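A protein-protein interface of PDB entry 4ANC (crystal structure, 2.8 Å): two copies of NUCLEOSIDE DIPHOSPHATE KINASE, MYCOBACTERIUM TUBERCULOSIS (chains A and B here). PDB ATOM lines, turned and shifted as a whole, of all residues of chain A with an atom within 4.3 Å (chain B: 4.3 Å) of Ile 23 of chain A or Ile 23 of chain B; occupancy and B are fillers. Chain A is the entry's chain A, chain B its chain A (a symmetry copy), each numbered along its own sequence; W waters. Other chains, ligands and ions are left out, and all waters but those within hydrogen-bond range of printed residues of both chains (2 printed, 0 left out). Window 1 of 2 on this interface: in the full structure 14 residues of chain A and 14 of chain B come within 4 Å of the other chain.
Printed residues of chain B within 4 Å of Ile 23 of chain A: Gly 20 and Ile 23.
Printed residues of chain B within 4 Å of Ser 24 of chain A: Gly 20 (3.1 Å) and Glu 21 (3.1 Å).
Ile 9 of chain B touches none of the printed residues of chain A.
Printed residues of chain A within 4 Å of Gly 20 of chain B: Gly 20, Ile 23, Ser 24 and Glu 27.
Of the printed residues of chain A, Glu 21 of chain B touches Ser 24.
Printed residues of chain A within 4 Å of Ser 24 of chain B: Gly 20 (3.1 Å) and Glu 21 (3.1 Å).
Ile 33 of chain B touches none of the printed residues of chain A.
The nearest residue of chain B that does not touch Ile 23 of chain A is Ile 19 of chain B (4.1 Å).
The nearest residue of chain A that does not touch Ile 23 of chain B is Ile 19 of chain A (4.1 Å).
Ile 19 of chain A touches Glu 27 of chain B, and with the chains exchanged Glu 27 of chain A touches Ile 19 of chain B.
Gly 20 of chain B touches its own counterpart, Gly 20 of chain A.
Gly 20 of chain A touches Ile 23 of chain B, and with the chains exchanged Ile 23 of chain A touches Gly 20 of chain B.
Gly 20 of chain A touches Glu 27 of chain B, and with the chains exchanged Glu 27 of chain A touches Gly 20 of chain B.
Positions printed for both chains: 9, 19, 20, 21, 22, 23, 24, 25, 26, 27 and 33.
Among the printed residues, pairs that only touch across the chains: Gly 20 of chain A with Ser 24 of chain B (3.1 Å), Ser 24 of chain A with Gly 20 of chain B (3.1 Å), Gly 20 of chain A with Ile 23 of chain B (3.8 Å), Ile 23 of chain A with Gly 20 of chain B (3.8 Å) and Ile 23 of chain A with Ile 23 of chain B (3.8 Å).
The side-chain carboxylate (OE2) of Glu 21 of chain A lies within salt-bridge range of the guanidinium group (NE) of Arg 25 of chain A (3.0 Å).
The backbone carbonyl oxygen of Gly 20 of chain A sits at hydrogen-bond distance from the side-chain hydroxyl of Ser 24 of chain A (3.0 Å).
The side-chain hydroxyl (OG) of Ser 24 of chain B is in hydrogen-bond range of the backbone carbonyl oxygen (O) of Gly 20 of chain B, at 3.0 Å.
NE of Arg 25 of chain B is in salt-bridge range of OE2 of Glu 21 of chain B.
Printed residues of chain A that touch a printed residue of chain B: Ile 19, Gly 20, Glu 21, Ile 23, Ser 24 and Glu 27.
Of the 11 printed residues of chain B, 6 touch a printed residue of chain A.
Hydrophobic or aromatic side chains of chain B within 4 Å of the printed part of chain A: Ile 19 and Ile 23.
Among the printed residues, no Asp or Glu carboxylate lies within 4 Å of a Lys or Arg side-chain nitrogen of the other chain.
Water W1 lies within hydrogen-bond range of OE1 of Glu 27 of chain B, OG of Ser 24 of chain B, N of Glu 21 of chain A and N of Gly 20 of chain A.
Water W2 lies within hydrogen-bond range of OE1 of Glu 27 of chain A, OG of Ser 24 of chain A, N of Glu 21 of chain B and N of Gly 20 of chain B.
N of Gly 20 of chain A lies within hydrogen-bond range of OE1 of Glu 27 of chain B.
The side-chain carboxylate (OE1) of Glu 27 of chain A is in hydrogen-bond range of the backbone NH (N) of Gly 20 of chain B (2.9 Å).
N of Glu 21 of chain B lies within hydrogen-bond range of OG of Ser 24 of chain A, at 3.1 Å.
The backbone NH of Ile 19 of chain B lies within hydrogen-bond range of the side-chain carboxylate of Glu 27 of chain A, at 3.3 Å.
O of Gly 20 of chain A sits close to O of Gly 20 of chain B, 3.4 Å away.
The backbone NH (N) of Ile 19 of chain A lies within hydrogen-bond range of the side-chain carboxylate (OE2) of Glu 27 of chain B, at 3.3 Å.
OG of Ser 24 of chain B sits at hydrogen-bond distance from N of Glu 21 of chain A, 3.1 Å away.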
ATOM      1  N   ILE A   9     -16.853 -18.189   3.469  1.00  0.00           N
ATOM      2  CA  ILE A   9     -17.524 -18.064   4.753  1.00  0.00           C
ATOM      3  C   ILE A   9     -18.974 -18.460   4.511  1.00  0.00           C
ATOM      4  O   ILE A   9     -19.745 -17.711   3.914  1.00  0.00           O
ATOM      5  CB  ILE A   9     -17.436 -16.639   5.322  1.00  0.00           C
ATOM      6  CG1 ILE A   9     -15.972 -16.201   5.433  1.00  0.00           C
ATOM      7  CG2 ILE A   9     -18.121 -16.567   6.681  1.00  0.00           C
ATOM      8  CD1 ILE A   9     -15.786 -14.791   5.974  1.00  0.00           C
ATOM      9  N   ILE A  19     -18.187 -13.050  10.058  1.00  0.00           N
ATOM     10  CA  ILE A  19     -17.514 -12.587   8.850  1.00  0.00           C
ATOM     11  C   ILE A  19     -16.234 -11.839   9.205  1.00  0.00           C
ATOM     12  O   ILE A  19     -15.144 -12.213   8.772  1.00  0.00           O
ATOM     13  CB  ILE A  19     -18.420 -11.658   8.012  1.00  0.00           C
ATOM     14  CG1 ILE A  19     -19.744 -12.350   7.675  1.00  0.00           C
ATOM     15  CG2 ILE A  19     -17.704 -11.224   6.740  1.00  0.00           C
ATOM     16  CD1 ILE A  19     -20.667 -11.519   6.800  1.00  0.00           C
ATOM     17  N   GLY A  20     -16.377 -10.780   9.998  1.00  0.00           N
ATOM     18  CA  GLY A  20     -15.252  -9.957  10.402  1.00  0.00           C
ATOM     19  C   GLY A  20     -14.248 -10.691  11.269  1.00  0.00           C
ATOM     20  O   GLY A  20     -13.047 -10.465  11.161  1.00  0.00           O
ATOM     21  N   GLU A  21     -14.739 -11.571  12.134  1.00  0.00           N
ATOM     22  CA  GLU A  21     -13.864 -12.370  12.984  1.00  0.00           C
ATOM     23  C   GLU A  21     -12.932 -13.239  12.148  1.00  0.00           C
ATOM     24  O   GLU A  21     -11.731 -13.306  12.405  1.00  0.00           O
ATOM     25  CB  GLU A  21     -14.681 -13.247  13.935  1.00  0.00           C
ATOM     26  CG  GLU A  21     -13.834 -14.217  14.762  1.00  0.00           C
ATOM     27  CD  GLU A  21     -12.938 -13.517  15.767  1.00  0.00           C
ATOM     28  OE1 GLU A  21     -13.202 -12.335  16.076  1.00  0.00           O
ATOM     29  OE2 GLU A  21     -11.970 -14.154  16.239  1.00  0.00           O
ATOM     30  N   ILE A  22     -13.495 -13.903  11.145  1.00  0.00           N
ATOM     31  CA  ILE A  22     -12.723 -14.767  10.260  1.00  0.00           C
ATOM     32  C   ILE A  22     -11.733 -13.962   9.418  1.00  0.00           C
ATOM     33  O   ILE A  22     -10.536 -14.262   9.394  1.00  0.00           O
ATOM     34  CB  ILE A  22     -13.646 -15.570   9.332  1.00  0.00           C
ATOM     35  CG1 ILE A  22     -14.505 -16.544  10.146  1.00  0.00           C
ATOM     36  CG2 ILE A  22     -12.831 -16.312   8.293  1.00  0.00           C
ATOM     37  CD1 ILE A  22     -15.645 -17.159   9.360  1.00  0.00           C
ATOM     38  N   ILE A  23     -12.238 -12.941   8.732  1.00  0.00           N
ATOM     39  CA  ILE A  23     -11.397 -12.062   7.926  1.00  0.00           C
ATOM     40  C   ILE A  23     -10.245 -11.503   8.754  1.00  0.00           C
ATOM     41  O   ILE A  23      -9.098 -11.485   8.309  1.00  0.00           O
ATOM     42  CB  ILE A  23     -12.210 -10.893   7.336  1.00  0.00           C
ATOM     43  CG1 ILE A  23     -13.268 -11.420   6.365  1.00  0.00           C
ATOM     44  CG2 ILE A  23     -11.294  -9.899   6.635  1.00  0.00           C
ATOM     45  CD1 ILE A  23     -14.136 -10.340   5.770  1.00  0.00           C
ATOM     46  N   SER A  24     -10.558 -11.050   9.964  1.00  0.00           N
ATOM     47  CA  SER A  24      -9.544 -10.521  10.870  1.00  0.00           C
ATOM     48  C   SER A  24      -8.409 -11.513  11.103  1.00  0.00           C
ATOM     49  O   SER A  24      -7.239 -11.169  10.945  1.00  0.00           O
ATOM     50  CB  SER A  24     -10.166 -10.108  12.208  1.00  0.00           C
ATOM     51  OG  SER A  24     -10.779  -8.833  12.112  1.00  0.00           O
ATOM     52  N   ARG A  25      -8.755 -12.741  11.483  1.00  0.00           N
ATOM     53  CA  ARG A  25      -7.753 -13.781  11.712  1.00  0.00           C
ATOM     54  C   ARG A  25      -6.837 -13.945  10.498  1.00  0.00           C
ATOM     55  O   ARG A  25      -5.624 -14.108  10.641  1.00  0.00           O
ATOM     56  CB  ARG A  25      -8.416 -15.122  12.052  1.00  0.00           C
ATOM     57  CG  ARG A  25      -9.377 -15.071  13.239  1.00  0.00           C
ATOM     58  CD  ARG A  25      -9.528 -16.445  13.910  1.00  0.00           C
ATOM     59  NE  ARG A  25     -10.453 -16.397  15.041  1.00  0.00           N
ATOM     60  CZ  ARG A  25     -10.502 -17.307  16.010  1.00  0.00           C
ATOM     61  NH1 ARG A  25      -9.670 -18.341  16.001  1.00  0.00           N
ATOM     62  NH2 ARG A  25     -11.381 -17.180  16.996  1.00  0.00           N
ATOM     63  N   ILE A  26      -7.423 -13.909   9.307  1.00  0.00           N
ATOM     64  CA  ILE A  26      -6.654 -13.995   8.071  1.00  0.00           C
ATOM     65  C   ILE A  26      -5.702 -12.810   7.958  1.00  0.00           C
ATOM     66  O   ILE A  26      -4.492 -12.981   7.812  1.00  0.00           O
ATOM     67  CB  ILE A  26      -7.580 -14.045   6.842  1.00  0.00           C
ATOM     68  CG1 ILE A  26      -8.378 -15.353   6.834  1.00  0.00           C
ATOM     69  CG2 ILE A  26      -6.775 -13.916   5.560  1.00  0.00           C
ATOM     70  CD1 ILE A  26      -9.492 -15.387   5.809  1.00  0.00           C
ATOM     71  N   GLU A  27      -6.262 -11.609   8.048  1.00  0.00           N
ATOM     72  CA  GLU A  27      -5.474 -10.383   8.022  1.00  0.00           C
ATOM     73  C   GLU A  27      -4.319 -10.442   9.019  1.00  0.00           C
ATOM     74  O   GLU A  27      -3.165 -10.187   8.665  1.00  0.00           O
ATOM     75  CB  GLU A  27      -6.358  -9.172   8.330  1.00  0.00           C
ATOM     76  CG  GLU A  27      -7.381  -8.857   7.257  1.00  0.00           C
ATOM     77  CD  GLU A  27      -8.169  -7.599   7.564  1.00  0.00           C
ATOM     78  OE1 GLU A  27      -9.093  -7.663   8.402  1.00  0.00           O
ATOM     79  OE2 GLU A  27      -7.868  -6.548   6.960  1.00  0.00           O
ATOM     80  N   ILE A  33      -6.394 -10.013   1.597  1.00  0.00           N
ATOM     81  CA  ILE A  33      -7.621 -10.256   0.856  1.00  0.00           C
ATOM     82  C   ILE A  33      -7.484  -9.700  -0.558  1.00  0.00           C
ATOM     83  O   ILE A  33      -7.458  -8.486  -0.755  1.00  0.00           O
ATOM     84  CB  ILE A  33      -8.839  -9.622   1.565  1.00  0.00           C
ATOM     85  CG1 ILE A  33      -9.250 -10.456   2.782  1.00  0.00           C
ATOM     86  CG2 ILE A  33     -10.016  -9.492   0.609  1.00  0.00           C
ATOM     87  CD1 ILE A  33      -8.220 -10.492   3.886  1.00  0.00           C
ATOM     88  N   ILE B   9     -14.958   0.847   3.328  1.00  0.00           N
ATOM     89  CA  ILE B   9     -13.696   0.678   4.031  1.00  0.00           C
ATOM     90  C   ILE B   9     -12.608   1.100   3.054  1.00  0.00           C
ATOM     91  O   ILE B   9     -12.297   0.386   2.103  1.00  0.00           O
ATOM     92  CB  ILE B   9     -13.477  -0.770   4.498  1.00  0.00           C
ATOM     93  CG1 ILE B   9     -14.648  -1.231   5.372  1.00  0.00           C
ATOM     94  CG2 ILE B   9     -12.162  -0.889   5.259  1.00  0.00           C
ATOM     95  CD1 ILE B   9     -14.527  -2.663   5.868  1.00  0.00           C
ATOM     96  N   ILE B  19     -10.308  -4.540   7.907  1.00  0.00           N
ATOM     97  CA  ILE B  19     -11.535  -4.961   7.244  1.00  0.00           C
ATOM     98  C   ILE B  19     -12.424  -5.739   8.209  1.00  0.00           C
ATOM     99  O   ILE B  19     -13.569  -5.360   8.456  1.00  0.00           O
ATOM    100  CB  ILE B  19     -11.245  -5.844   6.010  1.00  0.00           C
ATOM    101  CG1 ILE B  19     -10.311  -5.123   5.034  1.00  0.00           C
ATOM    102  CG2 ILE B  19     -12.544  -6.235   5.319  1.00  0.00           C
ATOM    103  CD1 ILE B  19     -10.025  -5.907   3.764  1.00  0.00           C
ATOM    104  N   GLY B  20     -11.884  -6.827   8.751  1.00  0.00           N
ATOM    105  CA  GLY B  20     -12.617  -7.679   9.670  1.00  0.00           C
ATOM    106  C   GLY B  20     -12.977  -6.993  10.973  1.00  0.00           C
ATOM    107  O   GLY B  20     -14.044  -7.229  11.529  1.00  0.00           O
ATOM    108  N   GLU B  21     -12.083  -6.143  11.465  1.00  0.00           N
ATOM    109  CA  GLU B  21     -12.342  -5.391  12.687  1.00  0.00           C
ATOM    110  C   GLU B  21     -13.569  -4.499  12.530  1.00  0.00           C
ATOM    111  O   GLU B  21     -14.434  -4.457  13.403  1.00  0.00           O
ATOM    112  CB  GLU B  21     -11.128  -4.543  13.073  1.00  0.00           C
ATOM    113  CG  GLU B  21     -11.375  -3.617  14.266  1.00  0.00           C
ATOM    114  CD  GLU B  21     -11.586  -4.369  15.568  1.00  0.00           C
ATOM    115  OE1 GLU B  21     -11.211  -5.559  15.635  1.00  0.00           O
ATOM    116  OE2 GLU B  21     -12.132  -3.763  16.518  1.00  0.00           O
ATOM    117  N   ILE B  22     -13.636  -3.788  11.410  1.00  0.00           N
ATOM    118  CA  ILE B  22     -14.755  -2.899  11.126  1.00  0.00           C
ATOM    119  C   ILE B  22     -16.054  -3.680  10.929  1.00  0.00           C
ATOM    120  O   ILE B  22     -17.067  -3.394  11.574  1.00  0.00           O
ATOM    121  CB  ILE B  22     -14.478  -2.048   9.879  1.00  0.00           C
ATOM    122  CG1 ILE B  22     -13.303  -1.097  10.131  1.00  0.00           C
ATOM    123  CG2 ILE B  22     -15.720  -1.274   9.483  1.00  0.00           C
ATOM    124  CD1 ILE B  22     -12.769  -0.436   8.876  1.00  0.00           C
ATOM    125  N   ILE B  23     -16.017  -4.667  10.037  1.00  0.00           N
ATOM    126  CA  ILE B  23     -17.172  -5.522   9.786  1.00  0.00           C
ATOM    127  C   ILE B  23     -17.693  -6.128  11.085  1.00  0.00           C
ATOM    128  O   ILE B  23     -18.897  -6.142  11.337  1.00  0.00           O
ATOM    129  CB  ILE B  23     -16.827  -6.656   8.800  1.00  0.00           C
ATOM    130  CG1 ILE B  23     -16.463  -6.078   7.432  1.00  0.00           C
ATOM    131  CG2 ILE B  23     -17.989  -7.632   8.674  1.00  0.00           C
ATOM    132  CD1 ILE B  23     -16.074  -7.122   6.417  1.00  0.00           C
ATOM    133  N   SER B  24     -16.776  -6.626  11.908  1.00  0.00           N
ATOM    134  CA  SER B  24     -17.138  -7.204  13.199  1.00  0.00           C
ATOM    135  C   SER B  24     -17.950  -6.236  14.053  1.00  0.00           C
ATOM    136  O   SER B  24     -19.021  -6.588  14.545  1.00  0.00           O
ATOM    137  CB  SER B  24     -15.891  -7.663  13.962  1.00  0.00           C
ATOM    138  OG  SER B  24     -15.446  -8.926  13.495  1.00  0.00           O
ATOM    139  N   ARG B  25     -17.438  -5.020  14.233  1.00  0.00           N
ATOM    140  CA  ARG B  25     -18.141  -4.002  15.013  1.00  0.00           C
ATOM    141  C   ARG B  25     -19.568  -3.801  14.503  1.00  0.00           C
ATOM    142  O   ARG B  25     -20.504  -3.658  15.290  1.00  0.00           O
ATOM    143  CB  ARG B  25     -17.383  -2.668  14.991  1.00  0.00           C
ATOM    144  CG  ARG B  25     -15.931  -2.757  15.458  1.00  0.00           C
ATOM    145  CD  ARG B  25     -15.422  -1.409  15.993  1.00  0.00           C
ATOM    146  NE  ARG B  25     -14.030  -1.492  16.433  1.00  0.00           N
ATOM    147  CZ  ARG B  25     -13.449  -0.622  17.255  1.00  0.00           C
ATOM    148  NH1 ARG B  25     -14.139   0.402  17.743  1.00  0.00           N
ATOM    149  NH2 ARG B  25     -12.176  -0.778  17.595  1.00  0.00           N
ATOM    150  N   ILE B  26     -19.727  -3.781  13.185  1.00  0.00           N
ATOM    151  CA  ILE B  26     -21.045  -3.655  12.573  1.00  0.00           C
ATOM    152  C   ILE B  26     -21.918  -4.845  12.950  1.00  0.00           C
ATOM    153  O   ILE B  26     -23.010  -4.682  13.495  1.00  0.00           O
ATOM    154  CB  ILE B  26     -20.938  -3.543  11.041  1.00  0.00           C
ATOM    155  CG1 ILE B  26     -20.259  -2.226  10.652  1.00  0.00           C
ATOM    156  CG2 ILE B  26     -22.314  -3.630  10.401  1.00  0.00           C
ATOM    157  CD1 ILE B  26     -19.883  -2.138   9.188  1.00  0.00           C
ATOM    158  N   GLU B  27     -21.415  -6.042  12.671  1.00  0.00           N
ATOM    159  CA  GLU B  27     -22.104  -7.275  13.029  1.00  0.00           C
ATOM    160  C   GLU B  27     -22.528  -7.271  14.496  1.00  0.00           C
ATOM    161  O   GLU B  27     -23.690  -7.525  14.818  1.00  0.00           O
ATOM    162  CB  GLU B  27     -21.210  -8.487  12.755  1.00  0.00           C
ATOM    163  CG  GLU B  27     -20.941  -8.746  11.286  1.00  0.00           C
ATOM    164  CD  GLU B  27     -20.129 -10.005  11.062  1.00  0.00           C
ATOM    165  OE1 GLU B  27     -18.897  -9.965  11.262  1.00  0.00           O
ATOM    166  OE2 GLU B  27     -20.723 -11.035  10.678  1.00  0.00           O
ATOM    167  N   ILE B  33     -24.843  -7.372   7.133  1.00  0.00           N
ATOM    168  CA  ILE B  33     -24.215  -7.084   5.854  1.00  0.00           C
ATOM    169  C   ILE B  33     -25.108  -7.584   4.722  1.00  0.00           C
ATOM    170  O   ILE B  33     -25.252  -8.790   4.522  1.00  0.00           O
ATOM    171  CB  ILE B  33     -22.815  -7.732   5.757  1.00  0.00           C
ATOM    172  CG1 ILE B  33     -21.797  -6.943   6.586  1.00  0.00           C
ATOM    173  CG2 ILE B  33     -22.352  -7.809   4.309  1.00  0.00           C
ATOM    174  CD1 ILE B  33     -22.058  -6.964   8.073  1.00  0.00           C
HETATM  175  O   HOH W   1     -17.439 -10.977  13.309  1.00  0.00           O
HETATM  176  O   HOH W   2      -9.186  -6.752  10.951  1.00  0.00           O
